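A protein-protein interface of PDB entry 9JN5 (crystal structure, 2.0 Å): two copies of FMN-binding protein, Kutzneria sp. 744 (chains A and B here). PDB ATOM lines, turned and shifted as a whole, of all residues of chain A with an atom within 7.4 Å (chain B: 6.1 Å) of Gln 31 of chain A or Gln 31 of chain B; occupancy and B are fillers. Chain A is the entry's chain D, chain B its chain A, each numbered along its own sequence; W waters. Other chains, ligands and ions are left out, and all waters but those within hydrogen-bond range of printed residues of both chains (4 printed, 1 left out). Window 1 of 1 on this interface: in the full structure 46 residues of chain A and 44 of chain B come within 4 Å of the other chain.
The backbone carbonyl oxygen (O) of Ile 44 of chain B lies within hydrogen-bond range of the side-chain amide nitrogen (NE2) of Gln 118 of chain A, 3.2 Å away. The side-chain amide oxygen (OE1) of Gln 31 of chain A sits close to the side-chain amide oxygen (OE1) of Gln 31 of chain B, 3.2 Å away.
The backbone carbonyl oxygen (O) of Thr 90 of chain A lies within hydrogen-bond range of the backbone NH (N) of Gln 31 of chain A, at 2.8 Å. The backbone NH of Ala 33 of chain A lies within hydrogen-bond range of the backbone carbonyl oxygen of Val 88 of chain A. The backbone carbonyl oxygen of Thr 90 of chain B lies within hydrogen-bond range of the backbone NH of Gln 31 of chain B (3.0 Å). The side-chain amide nitrogen (NE2) of Gln 31 of chain B sits close to a ring nitrogen (NE2) of His 46 of chain B (3.3 Å). The backbone carbonyl oxygen (O) of Val 88 of chain B is in hydrogen-bond range of the backbone NH (N) of Ala 33 of chain B.
Among the printed residues, merely in contact across the chains: Thr 90 of chain A with Gln 31 of chain B (3.3 Å), Gln 31 of chain A with Thr 90 of chain B (3.4 Å), Val 88 of chain A with Ile 44 of chain B (3.7 Å), Ser 116 of chain A with His 46 of chain B (3.7 Å), Thr 90 of chain A with Ile 44 of chain B (3.7 Å), Ile 44 of chain A with Val 88 of chain B (3.8 Å), Ile 44 of chain A with Ala 33 of chain B (3.9 Å), His 46 of chain A with Thr 90 of chain B (3.9 Å), Thr 90 of chain A with His 46 of chain B (3.96 Å) and Ile 44 of chain A with Thr 90 of chain B (3.98 Å).
Gln 31 of chain A touches two residues of chain B. Printed residues of chain A within 4 Å of Gln 31 of chain B: Gln 31 and Thr 90. Printed residues of chain B within 4 Å of Ser 116 of chain A: His 46. Of the printed residues of chain B, Gln 118 of chain A touches Ile 44. Of the printed residues of chain B, Val 88 of chain A touches Ile 44. Of the printed residues of chain A, Ala 33 of chain B touches Ile 44 (3.9 Å). Leu 29 of chain B touches none of the printed residues of chain A. Ala 30 of chain B touches none of the printed residues of chain A. The nearest residue of chain B that does not touch Gln 31 of chain A is Ala 92 of chain B (4.2 Å). The nearest residue of chain A that does not touch Gln 31 of chain B is Ala 92 of chain A (4.2 Å). The nearest printed residue of chain B that does not touch Ile 44 of chain A is Ile 44 of chain B (4.8 Å).
Among the printed residues, 12 pairs touch across the chains. Among the printed residues, no Asp or Glu carboxylate lies within 4 Å of a Lys or Arg side-chain nitrogen of the other chain.
Gln 31 of chain A touches Thr 90 of chain B, and with the chains exchanged Thr 90 of chain A touches Gln 31 of chain B. Ile 44 of chain A touches Ala 33 of chain B, but with the chains exchanged Ala 33 of chain A does not touch Ile 44 of chain B (4.1 Å). Ile 44 of chain A touches Val 88 of chain B, and with the chains exchanged Val 88 of chain A touches Ile 44 of chain B. His 46 of chain A touches Thr 90 of chain B, and with the chains exchanged Thr 90 of chain A touches His 46 of chain B. Of the 12 pairs that touch across the chains among the printed residues, 9 have their exchanged pair printed and touching as well.
Water W2 bridges OE1 of Gln 31 of chain B and OE1 of Gln 31 of chain A. Water W1 lies within hydrogen-bond range of the backbone carbonyl oxygen (O) of Thr 90 of chain A (2.7 Å) and the side-chain amide nitrogen (NE2) of Gln 31 of chain B (3.0 Å). Water W4 lies within hydrogen-bond range of the backbone carbonyl oxygen of Ile 44 of chain B and the side-chain amide oxygen of Gln 118 of chain A. Water W3 bridges the backbone carbonyl oxygen (O) of Thr 90 of chain B (2.7 Å) and the side-chain amide nitrogen (NE2) of Gln 31 of chain A (2.8 Å).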
ATOM      1  N   HIS A  27     -16.779 -24.075  23.865  1.00  0.00           N
ATOM      2  CA  HIS A  27     -15.631 -23.284  23.313  1.00  0.00           C
ATOM      3  C   HIS A  27     -14.382 -24.155  23.299  1.00  0.00           C
ATOM      4  O   HIS A  27     -13.381 -23.908  23.960  1.00  0.00           O
ATOM      5  CB  HIS A  27     -15.523 -21.976  24.086  1.00  0.00           C
ATOM      6  CG  HIS A  27     -16.857 -21.346  24.259  1.00  0.00           C
ATOM      7  ND1 HIS A  27     -17.395 -20.500  23.306  1.00  0.00           N
ATOM      8  CD2 HIS A  27     -17.773 -21.443  25.242  1.00  0.00           C
ATOM      9  CE1 HIS A  27     -18.579 -20.095  23.710  1.00  0.00           C
ATOM     10  NE2 HIS A  27     -18.835 -20.652  24.885  1.00  0.00           N
ATOM     11  N   PRO A  28     -14.427 -25.225  22.499  1.00  0.00           N
ATOM     12  CA  PRO A  28     -13.398 -26.254  22.528  1.00  0.00           C
ATOM     13  C   PRO A  28     -12.046 -25.792  21.977  1.00  0.00           C
ATOM     14  O   PRO A  28     -11.083 -26.533  22.180  1.00  0.00           O
ATOM     15  CB  PRO A  28     -13.922 -27.350  21.610  1.00  0.00           C
ATOM     16  CG  PRO A  28     -14.965 -26.690  20.757  1.00  0.00           C
ATOM     17  CD  PRO A  28     -15.454 -25.469  21.495  1.00  0.00           C
ATOM     18  N   LEU A  29     -12.014 -24.631  21.317  1.00  0.00           N
ATOM     19  CA  LEU A  29     -10.766 -24.096  20.689  1.00  0.00           C
ATOM     20  C   LEU A  29     -10.006 -23.274  21.751  1.00  0.00           C
ATOM     21  O   LEU A  29     -10.214 -22.094  21.873  1.00  0.00           O
ATOM     22  CB  LEU A  29     -11.051 -23.331  19.403  1.00  0.00           C
ATOM     23  CG  LEU A  29      -9.769 -23.045  18.606  1.00  0.00           C
ATOM     24  CD1 LEU A  29      -9.294 -24.294  17.871  1.00  0.00           C
ATOM     25  CD2 LEU A  29      -9.879 -21.851  17.661  1.00  0.00           C
ATOM     26  N   ALA A  30      -9.201 -23.969  22.550  1.00  0.00           N
ATOM     27  CA  ALA A  30      -8.527 -23.443  23.746  1.00  0.00           C
ATOM     28  C   ALA A  30      -7.230 -22.778  23.329  1.00  0.00           C
ATOM     29  O   ALA A  30      -6.690 -23.105  22.228  1.00  0.00           O
ATOM     30  CB  ALA A  30      -8.274 -24.566  24.715  1.00  0.00           C
ATOM     31  N   GLN A  31      -6.716 -21.914  24.192  1.00  0.00           N
ATOM     32  CA  GLN A  31      -5.322 -21.423  24.060  1.00  0.00           C
ATOM     33  C   GLN A  31      -4.445 -22.257  24.998  1.00  0.00           C
ATOM     34  O   GLN A  31      -4.691 -22.272  26.230  1.00  0.00           O
ATOM     35  CB  GLN A  31      -5.212 -19.925  24.335  1.00  0.00           C
ATOM     36  CG  GLN A  31      -5.980 -19.039  23.361  1.00  0.00           C
ATOM     37  CD  GLN A  31      -5.723 -17.565  23.637  1.00  0.00           C
ATOM     38  OE1 GLN A  31      -4.688 -17.187  24.196  1.00  0.00           O
ATOM     39  NE2 GLN A  31      -6.669 -16.724  23.260  1.00  0.00           N
ATOM     40  N   LEU A  32      -3.538 -23.029  24.409  1.00  0.00           N
ATOM     41  CA  LEU A  32      -2.638 -23.938  25.159  1.00  0.00           C
ATOM     42  C   LEU A  32      -1.319 -23.205  25.418  1.00  0.00           C
ATOM     43  O   LEU A  32      -0.669 -22.841  24.450  1.00  0.00           O
ATOM     44  CB  LEU A  32      -2.414 -25.226  24.360  1.00  0.00           C
ATOM     45  CG  LEU A  32      -1.454 -26.217  25.022  1.00  0.00           C
ATOM     46  CD1 LEU A  32      -2.073 -26.839  26.256  1.00  0.00           C
ATOM     47  CD2 LEU A  32      -1.017 -27.307  24.047  1.00  0.00           C
ATOM     48  N   ALA A  33      -0.957 -22.996  26.682  1.00  0.00           N
ATOM     49  CA  ALA A  33       0.256 -22.237  27.082  1.00  0.00           C
ATOM     50  C   ALA A  33       1.205 -23.145  27.876  1.00  0.00           C
ATOM     51  O   ALA A  33       0.735 -23.875  28.749  1.00  0.00           O
ATOM     52  CB  ALA A  33      -0.118 -21.008  27.887  1.00  0.00           C
ATOM     53  N   SER A  34       2.500 -23.042  27.604  1.00  0.00           N
ATOM     54  CA  SER A  34       3.596 -23.667  28.380  1.00  0.00           C
ATOM     55  C   SER A  34       4.754 -22.664  28.400  1.00  0.00           C
ATOM     56  O   SER A  34       4.785 -21.788  27.546  1.00  0.00           O
ATOM     57  CB  SER A  34       3.989 -24.971  27.774  1.00  0.00           C
ATOM     58  OG  SER A  34       4.528 -24.771  26.462  1.00  0.00           O
ATOM     59  N   HIS A  43       4.959 -20.234  24.937  1.00  0.00           N
ATOM     60  CA  HIS A  43       4.347 -20.724  23.667  1.00  0.00           C
ATOM     61  C   HIS A  43       2.839 -20.772  23.839  1.00  0.00           C
ATOM     62  O   HIS A  43       2.380 -21.209  24.914  1.00  0.00           O
ATOM     63  CB  HIS A  43       4.759 -22.140  23.272  1.00  0.00           C
ATOM     64  CG  HIS A  43       6.221 -22.308  23.145  1.00  0.00           C
ATOM     65  ND1 HIS A  43       6.834 -22.449  21.920  1.00  0.00           N
ATOM     66  CD2 HIS A  43       7.185 -22.382  24.090  1.00  0.00           C
ATOM     67  CE1 HIS A  43       8.128 -22.591  22.126  1.00  0.00           C
ATOM     68  NE2 HIS A  43       8.363 -22.545  23.450  1.00  0.00           N
ATOM     69  N   ILE A  44       2.106 -20.278  22.849  1.00  0.00           N
ATOM     70  CA  ILE A  44       0.619 -20.295  22.874  1.00  0.00           C
ATOM     71  C   ILE A  44       0.147 -20.872  21.538  1.00  0.00           C
ATOM     72  O   ILE A  44       0.586 -20.380  20.466  1.00  0.00           O
ATOM     73  CB  ILE A  44       0.033 -18.895  23.100  1.00  0.00           C
ATOM     74  CG1 ILE A  44       0.633 -18.165  24.301  1.00  0.00           C
ATOM     75  CG2 ILE A  44      -1.475 -19.015  23.167  1.00  0.00           C
ATOM     76  CD1 ILE A  44      -0.084 -18.401  25.586  1.00  0.00           C
ATOM     77  N   THR A  45      -0.690 -21.901  21.586  1.00  0.00           N
ATOM     78  CA  THR A  45      -1.255 -22.534  20.372  1.00  0.00           C
ATOM     79  C   THR A  45      -2.755 -22.691  20.577  1.00  0.00           C
ATOM     80  O   THR A  45      -3.107 -23.205  21.631  1.00  0.00           O
ATOM     81  CB  THR A  45      -0.598 -23.881  20.063  1.00  0.00           C
ATOM     82  OG1 THR A  45       0.813 -23.708  20.081  1.00  0.00           O
ATOM     83  CG2 THR A  45      -1.044 -24.414  18.717  1.00  0.00           C
ATOM     84  N   HIS A  46      -3.561 -22.233  19.606  1.00  0.00           N
ATOM     85  CA  HIS A  46      -5.013 -22.520  19.525  1.00  0.00           C
ATOM     86  C   HIS A  46      -5.188 -23.970  19.129  1.00  0.00           C
ATOM     87  O   HIS A  46      -4.761 -24.358  18.042  1.00  0.00           O
ATOM     88  CB  HIS A  46      -5.729 -21.574  18.582  1.00  0.00           C
ATOM     89  CG  HIS A  46      -5.888 -20.216  19.162  1.00  0.00           C
ATOM     90  ND1 HIS A  46      -4.886 -19.274  19.083  1.00  0.00           N
ATOM     91  CD2 HIS A  46      -6.907 -19.656  19.847  1.00  0.00           C
ATOM     92  CE1 HIS A  46      -5.292 -18.179  19.694  1.00  0.00           C
ATOM     93  NE2 HIS A  46      -6.529 -18.381  20.161  1.00  0.00           N
ATOM     94  N   VAL A  47      -5.726 -24.749  20.040  1.00  0.00           N
ATOM     95  CA  VAL A  47      -5.888 -26.228  19.867  1.00  0.00           C
ATOM     96  C   VAL A  47      -7.298 -26.609  20.224  1.00  0.00           C
ATOM     97  O   VAL A  47      -7.818 -26.166  21.241  1.00  0.00           O
ATOM     98  CB  VAL A  47      -4.916 -27.056  20.727  1.00  0.00           C
ATOM     99  CG1 VAL A  47      -3.495 -26.961  20.200  1.00  0.00           C
ATOM    100  CG2 VAL A  47      -4.993 -26.700  22.207  1.00  0.00           C
ATOM    101  N   ILE A  49      -9.894 -29.017  21.924  1.00  0.00           N
ATOM    102  CA  ILE A  49      -9.809 -29.863  23.141  1.00  0.00           C
ATOM    103  C   ILE A  49     -11.215 -30.293  23.571  1.00  0.00           C
ATOM    104  O   ILE A  49     -12.076 -29.434  23.658  1.00  0.00           O
ATOM    105  CB  ILE A  49      -9.061 -29.124  24.278  1.00  0.00           C
ATOM    106  CG1 ILE A  49      -7.642 -28.711  23.845  1.00  0.00           C
ATOM    107  CG2 ILE A  49      -9.061 -29.969  25.538  1.00  0.00           C
ATOM    108  CD1 ILE A  49      -6.804 -28.212  24.966  1.00  0.00           C
ATOM    109  N   HIS A  77       6.019 -25.693  19.155  1.00  0.00           N
ATOM    110  CA  HIS A  77       5.330 -25.864  20.460  1.00  0.00           C
ATOM    111  C   HIS A  77       5.305 -27.363  20.786  1.00  0.00           C
ATOM    112  O   HIS A  77       5.552 -27.736  21.956  1.00  0.00           O
ATOM    113  CB  HIS A  77       3.964 -25.179  20.418  1.00  0.00           C
ATOM    114  CG  HIS A  77       3.366 -25.008  21.769  1.00  0.00           C
ATOM    115  ND1 HIS A  77       2.164 -24.383  21.954  1.00  0.00           N
ATOM    116  CD2 HIS A  77       3.813 -25.347  22.990  1.00  0.00           C
ATOM    117  CE1 HIS A  77       1.875 -24.384  23.226  1.00  0.00           C
ATOM    118  NE2 HIS A  77       2.880 -24.916  23.878  1.00  0.00           N
ATOM    119  N   VAL A  88      -1.263 -24.855  30.912  1.00  0.00           N
ATOM    120  CA  VAL A  88      -2.616 -24.280  31.128  1.00  0.00           C
ATOM    121  C   VAL A  88      -3.271 -24.278  29.762  1.00  0.00           C
ATOM    122  O   VAL A  88      -2.551 -24.019  28.729  1.00  0.00           O
ATOM    123  CB  VAL A  88      -2.577 -22.870  31.734  1.00  0.00           C
ATOM    124  CG1 VAL A  88      -1.674 -21.938  30.937  1.00  0.00           C
ATOM    125  CG2 VAL A  88      -3.979 -22.297  31.830  1.00  0.00           C
ATOM    126  N   ALA A  89      -4.535 -24.659  29.728  1.00  0.00           N
ATOM    127  CA  ALA A  89      -5.371 -24.478  28.525  1.00  0.00           C
ATOM    128  C   ALA A  89      -6.483 -23.541  28.945  1.00  0.00           C
ATOM    129  O   ALA A  89      -7.110 -23.850  29.982  1.00  0.00           O
ATOM    130  CB  ALA A  89      -5.864 -25.811  28.027  1.00  0.00           C
ATOM    131  N   THR A  90      -6.664 -22.418  28.238  1.00  0.00           N
ATOM    132  CA  THR A  90      -7.685 -21.384  28.551  1.00  0.00           C
ATOM    133  C   THR A  90      -8.799 -21.432  27.497  1.00  0.00           C
ATOM    134  O   THR A  90      -8.517 -21.427  26.298  1.00  0.00           O
ATOM    135  CB  THR A  90      -7.073 -19.992  28.644  1.00  0.00           C
ATOM    136  OG1 THR A  90      -5.965 -20.067  29.549  1.00  0.00           O
ATOM    137  CG2 THR A  90      -8.061 -18.936  29.103  1.00  0.00           C
ATOM    138  N   PHE A  91     -10.021 -21.496  27.962  1.00  0.00           N
ATOM    139  CA  PHE A  91     -11.235 -21.620  27.139  1.00  0.00           C
ATOM    140  C   PHE A  91     -12.021 -20.330  27.339  1.00  0.00           C
ATOM    141  O   PHE A  91     -12.300 -20.023  28.495  1.00  0.00           O
ATOM    142  CB  PHE A  91     -12.059 -22.810  27.601  1.00  0.00           C
ATOM    143  CG  PHE A  91     -11.398 -24.146  27.475  1.00  0.00           C
ATOM    144  CD1 PHE A  91     -10.553 -24.622  28.476  1.00  0.00           C
ATOM    145  CD2 PHE A  91     -11.724 -24.986  26.426  1.00  0.00           C
ATOM    146  CE1 PHE A  91      -9.978 -25.876  28.366  1.00  0.00           C
ATOM    147  CE2 PHE A  91     -11.144 -26.239  26.320  1.00  0.00           C
ATOM    148  CZ  PHE A  91     -10.276 -26.681  27.290  1.00  0.00           C
ATOM    149  N   ALA A  92     -12.360 -19.625  26.273  1.00  0.00           N
ATOM    150  CA  ALA A  92     -12.948 -18.268  26.336  1.00  0.00           C
ATOM    151  C   ALA A  92     -14.396 -18.360  25.846  1.00  0.00           C
ATOM    152  O   ALA A  92     -14.583 -18.764  24.717  1.00  0.00           O
ATOM    153  CB  ALA A  92     -12.089 -17.308  25.527  1.00  0.00           C
ATOM    154  N   THR A 115     -16.325 -14.645  30.242  1.00  0.00           N
ATOM    155  CA  THR A 115     -16.275 -15.991  30.839  1.00  0.00           C
ATOM    156  C   THR A 115     -14.966 -16.627  30.389  1.00  0.00           C
ATOM    157  O   THR A 115     -14.618 -16.498  29.178  1.00  0.00           O
ATOM    158  CB  THR A 115     -17.496 -16.803  30.409  1.00  0.00           C
ATOM    159  OG1 THR A 115     -17.486 -16.772  28.980  1.00  0.00           O
ATOM    160  CG2 THR A 115     -18.790 -16.250  30.955  1.00  0.00           C
ATOM    161  N   SER A 116     -14.240 -17.247  31.310  1.00  0.00           N
ATOM    162  CA  SER A 116     -12.997 -17.988  30.967  1.00  0.00           C
ATOM    163  C   SER A 116     -12.899 -19.200  31.881  1.00  0.00           C
ATOM    164  O   SER A 116     -13.266 -19.059  33.069  1.00  0.00           O
ATOM    165  CB  SER A 116     -11.755 -17.131  31.134  1.00  0.00           C
ATOM    166  OG  SER A 116     -11.691 -16.722  32.499  1.00  0.00           O
ATOM    167  N   VAL A 117     -12.347 -20.295  31.378  1.00  0.00           N
ATOM    168  CA  VAL A 117     -11.948 -21.459  32.206  1.00  0.00           C
ATOM    169  C   VAL A 117     -10.486 -21.711  31.895  1.00  0.00           C
ATOM    170  O   VAL A 117     -10.150 -21.809  30.683  1.00  0.00           O
ATOM    171  CB  VAL A 117     -12.809 -22.697  31.934  1.00  0.00           C
ATOM    172  CG1 VAL A 117     -12.205 -23.967  32.522  1.00  0.00           C
ATOM    173  CG2 VAL A 117     -14.235 -22.502  32.430  1.00  0.00           C
ATOM    174  N   GLN A 118      -9.677 -21.815  32.945  1.00  0.00           N
ATOM    175  CA  GLN A 118      -8.249 -22.209  32.872  1.00  0.00           C
ATOM    176  C   GLN A 118      -8.058 -23.587  33.527  1.00  0.00           C
ATOM    177  O   GLN A 118      -8.322 -23.728  34.713  1.00  0.00           O
ATOM    178  CB  GLN A 118      -7.412 -21.113  33.535  1.00  0.00           C
ATOM    179  CG  GLN A 118      -7.389 -19.826  32.726  1.00  0.00           C
ATOM    180  CD  GLN A 118      -6.662 -18.710  33.410  1.00  0.00           C
ATOM    181  OE1 GLN A 118      -5.736 -18.934  34.162  1.00  0.00           O
ATOM    182  NE2 GLN A 118      -7.038 -17.491  33.083  1.00  0.00           N
ATOM    183  N   VAL A 119      -7.616 -24.583  32.783  1.00  0.00           N
ATOM    184  CA  VAL A 119      -7.348 -25.918  33.370  1.00  0.00           C
ATOM    185  C   VAL A 119      -5.838 -26.075  33.360  1.00  0.00           C
ATOM    186  O   VAL A 119      -5.244 -25.645  32.373  1.00  0.00           O
ATOM    187  CB  VAL A 119      -8.058 -27.065  32.629  1.00  0.00           C
ATOM    188  CG1 VAL A 119      -9.569 -26.952  32.773  1.00  0.00           C
ATOM    189  CG2 VAL A 119      -7.620 -27.160  31.172  1.00  0.00           C
ATOM    190  N   LEU B  29      -9.557  -7.197  24.778  1.00  0.00           N
ATOM    191  CA  LEU B  29      -9.443  -8.094  25.950  1.00  0.00           C
ATOM    192  C   LEU B  29      -8.510  -9.251  25.577  1.00  0.00           C
ATOM    193  O   LEU B  29      -8.979 -10.305  25.098  1.00  0.00           O
ATOM    194  CB  LEU B  29     -10.814  -8.557  26.435  1.00  0.00           C
ATOM    195  CG  LEU B  29     -10.769  -9.176  27.830  1.00  0.00           C
ATOM    196  CD1 LEU B  29     -10.449  -8.133  28.908  1.00  0.00           C
ATOM    197  CD2 LEU B  29     -12.063  -9.906  28.135  1.00  0.00           C
ATOM    198  N   ALA B  30      -7.217  -9.022  25.800  1.00  0.00           N
ATOM    199  CA  ALA B  30      -6.120  -9.960  25.508  1.00  0.00           C
ATOM    200  C   ALA B  30      -5.981 -10.968  26.648  1.00  0.00           C
ATOM    201  O   ALA B  30      -6.339 -10.654  27.772  1.00  0.00           O
ATOM    202  CB  ALA B  30      -4.837  -9.202  25.310  1.00  0.00           C
ATOM    203  N   GLN B  31      -5.413 -12.124  26.346  1.00  0.00           N
ATOM    204  CA  GLN B  31      -4.890 -13.083  27.353  1.00  0.00           C
ATOM    205  C   GLN B  31      -3.386 -12.813  27.501  1.00  0.00           C
ATOM    206  O   GLN B  31      -2.629 -13.089  26.545  1.00  0.00           O
ATOM    207  CB  GLN B  31      -5.242 -14.511  26.917  1.00  0.00           C
ATOM    208  CG  GLN B  31      -6.677 -14.977  27.271  1.00  0.00           C
ATOM    209  CD  GLN B  31      -6.942 -16.406  26.827  1.00  0.00           C
ATOM    210  OE1 GLN B  31      -6.118 -17.274  27.003  1.00  0.00           O
ATOM    211  NE2 GLN B  31      -8.036 -16.651  26.131  1.00  0.00           N
ATOM    212  N   LEU B  32      -2.986 -12.203  28.609  1.00  0.00           N
ATOM    213  CA  LEU B  32      -1.567 -11.871  28.920  1.00  0.00           C
ATOM    214  C   LEU B  32      -0.933 -13.098  29.586  1.00  0.00           C
ATOM    215  O   LEU B  32      -1.467 -13.531  30.632  1.00  0.00           O
ATOM    216  CB  LEU B  32      -1.480 -10.634  29.817  1.00  0.00           C
ATOM    217  CG  LEU B  32      -0.061 -10.143  30.148  1.00  0.00           C
ATOM    218  CD1 LEU B  32       0.694  -9.690  28.901  1.00  0.00           C
ATOM    219  CD2 LEU B  32      -0.071  -9.022  31.196  1.00  0.00           C
ATOM    220  N   ALA B  33       0.125 -13.670  28.975  1.00  0.00           N
ATOM    221  CA  ALA B  33       0.801 -14.874  29.501  1.00  0.00           C
ATOM    222  C   ALA B  33       2.261 -14.568  29.874  1.00  0.00           C
ATOM    223  O   ALA B  33       2.948 -13.904  29.124  1.00  0.00           O
ATOM    224  CB  ALA B  33       0.681 -16.009  28.509  1.00  0.00           C
ATOM    225  N   ILE B  44      -1.955 -16.625  33.318  1.00  0.00           N
ATOM    226  CA  ILE B  44      -2.864 -16.103  32.266  1.00  0.00           C
ATOM    227  C   ILE B  44      -3.842 -15.135  32.903  1.00  0.00           C
ATOM    228  O   ILE B  44      -4.519 -15.595  33.829  1.00  0.00           O
ATOM    229  CB  ILE B  44      -3.638 -17.263  31.644  1.00  0.00           C
ATOM    230  CG1 ILE B  44      -2.732 -18.392  31.178  1.00  0.00           C
ATOM    231  CG2 ILE B  44      -4.522 -16.752  30.543  1.00  0.00           C
ATOM    232  CD1 ILE B  44      -1.803 -17.990  30.066  1.00  0.00           C
ATOM    233  N   THR B  45      -3.903 -13.876  32.430  1.00  0.00           N
ATOM    234  CA  THR B  45      -4.903 -12.873  32.864  1.00  0.00           C
ATOM    235  C   THR B  45      -5.501 -12.205  31.632  1.00  0.00           C
ATOM    236  O   THR B  45      -4.739 -11.778  30.749  1.00  0.00           O
ATOM    237  CB  THR B  45      -4.325 -11.806  33.807  1.00  0.00           C
ATOM    238  OG1 THR B  45      -3.587 -12.453  34.861  1.00  0.00           O
ATOM    239  CG2 THR B  45      -5.403 -10.934  34.416  1.00  0.00           C
ATOM    240  N   HIS B  46      -6.830 -12.147  31.598  1.00  0.00           N
ATOM    241  CA  HIS B  46      -7.626 -11.374  30.612  1.00  0.00           C
ATOM    242  C   HIS B  46      -7.485  -9.896  30.990  1.00  0.00           C
ATOM    243  O   HIS B  46      -7.913  -9.502  32.064  1.00  0.00           O
ATOM    244  CB  HIS B  46      -9.086 -11.874  30.537  1.00  0.00           C
ATOM    245  CG  HIS B  46      -9.282 -13.052  29.628  1.00  0.00           C
ATOM    246  ND1 HIS B  46      -9.147 -14.358  30.060  1.00  0.00           N
ATOM    247  CD2 HIS B  46      -9.598 -13.131  28.318  1.00  0.00           C
ATOM    248  CE1 HIS B  46      -9.347 -15.195  29.049  1.00  0.00           C
ATOM    249  NE2 HIS B  46      -9.659 -14.470  27.984  1.00  0.00           N
ATOM    250  N   VAL B  47      -6.851  -9.114  30.139  1.00  0.00           N
ATOM    251  CA  VAL B  47      -6.531  -7.693  30.443  1.00  0.00           C
ATOM    252  C   VAL B  47      -6.874  -6.847  29.223  1.00  0.00           C
ATOM    253  O   VAL B  47      -6.612  -7.274  28.089  1.00  0.00           O
ATOM    254  CB  VAL B  47      -5.056  -7.543  30.861  1.00  0.00           C
ATOM    255  CG1 VAL B  47      -4.774  -8.193  32.205  1.00  0.00           C
ATOM    256  CG2 VAL B  47      -4.102  -8.079  29.800  1.00  0.00           C
ATOM    257  N   VAL B  88       3.779 -12.591  26.346  1.00  0.00           N
ATOM    258  CA  VAL B  88       2.982 -12.704  25.095  1.00  0.00           C
ATOM    259  C   VAL B  88       1.590 -12.220  25.469  1.00  0.00           C
ATOM    260  O   VAL B  88       1.117 -12.575  26.540  1.00  0.00           O
ATOM    261  CB  VAL B  88       3.002 -14.119  24.493  1.00  0.00           C
ATOM    262  CG1 VAL B  88       2.732 -15.190  25.536  1.00  0.00           C
ATOM    263  CG2 VAL B  88       2.035 -14.262  23.344  1.00  0.00           C
ATOM    264  N   ALA B  89       0.998 -11.377  24.635  1.00  0.00           N
ATOM    265  CA  ALA B  89      -0.417 -10.990  24.766  1.00  0.00           C
ATOM    266  C   ALA B  89      -1.129 -11.485  23.513  1.00  0.00           C
ATOM    267  O   ALA B  89      -0.617 -11.222  22.397  1.00  0.00           O
ATOM    268  CB  ALA B  89      -0.523  -9.503  24.956  1.00  0.00           C
ATOM    269  N   THR B  90      -2.147 -12.321  23.690  1.00  0.00           N
ATOM    270  CA  THR B  90      -2.862 -12.976  22.570  1.00  0.00           C
ATOM    271  C   THR B  90      -4.244 -12.317  22.422  1.00  0.00           C
ATOM    272  O   THR B  90      -5.053 -12.243  23.416  1.00  0.00           O
ATOM    273  CB  THR B  90      -2.948 -14.488  22.770  1.00  0.00           C
ATOM    274  OG1 THR B  90      -1.644 -15.055  22.832  1.00  0.00           O
ATOM    275  CG2 THR B  90      -3.698 -15.142  21.636  1.00  0.00           C
ATOM    276  N   PHE B  91      -4.496 -11.786  21.252  1.00  0.00           N
ATOM    277  CA  PHE B  91      -5.805 -11.207  20.892  1.00  0.00           C
ATOM    278  C   PHE B  91      -6.489 -12.251  20.008  1.00  0.00           C
ATOM    279  O   PHE B  91      -5.866 -12.735  19.032  1.00  0.00           O
ATOM    280  CB  PHE B  91      -5.587  -9.855  20.223  1.00  0.00           C
ATOM    281  CG  PHE B  91      -4.788  -8.856  21.025  1.00  0.00           C
ATOM    282  CD1 PHE B  91      -3.398  -8.944  21.131  1.00  0.00           C
ATOM    283  CD2 PHE B  91      -5.423  -7.776  21.621  1.00  0.00           C
ATOM    284  CE1 PHE B  91      -2.672  -7.985  21.812  1.00  0.00           C
ATOM    285  CE2 PHE B  91      -4.685  -6.774  22.236  1.00  0.00           C
ATOM    286  CZ  PHE B  91      -3.323  -6.927  22.399  1.00  0.00           C
ATOM    287  N   ALA B  92      -7.738 -12.543  20.309  1.00  0.00           N
ATOM    288  CA  ALA B  92      -8.552 -13.538  19.588  1.00  0.00           C
ATOM    289  C   ALA B  92      -9.718 -12.838  18.868  1.00  0.00           C
ATOM    290  O   ALA B  92     -10.608 -12.281  19.535  1.00  0.00           O
ATOM    291  CB  ALA B  92      -9.008 -14.575  20.573  1.00  0.00           C
HETATM  292  O   HOH W   1      -9.030 -19.198  24.897  1.00  0.00           O
HETATM  293  O   HOH W   2      -3.553 -17.726  26.736  1.00  0.00           O
HETATM  294  O   HOH W   3      -7.131 -14.017  23.560  1.00  0.00           O
HETATM  295  O   HOH W   4      -3.288 -17.251  35.624  1.00  0.00           O
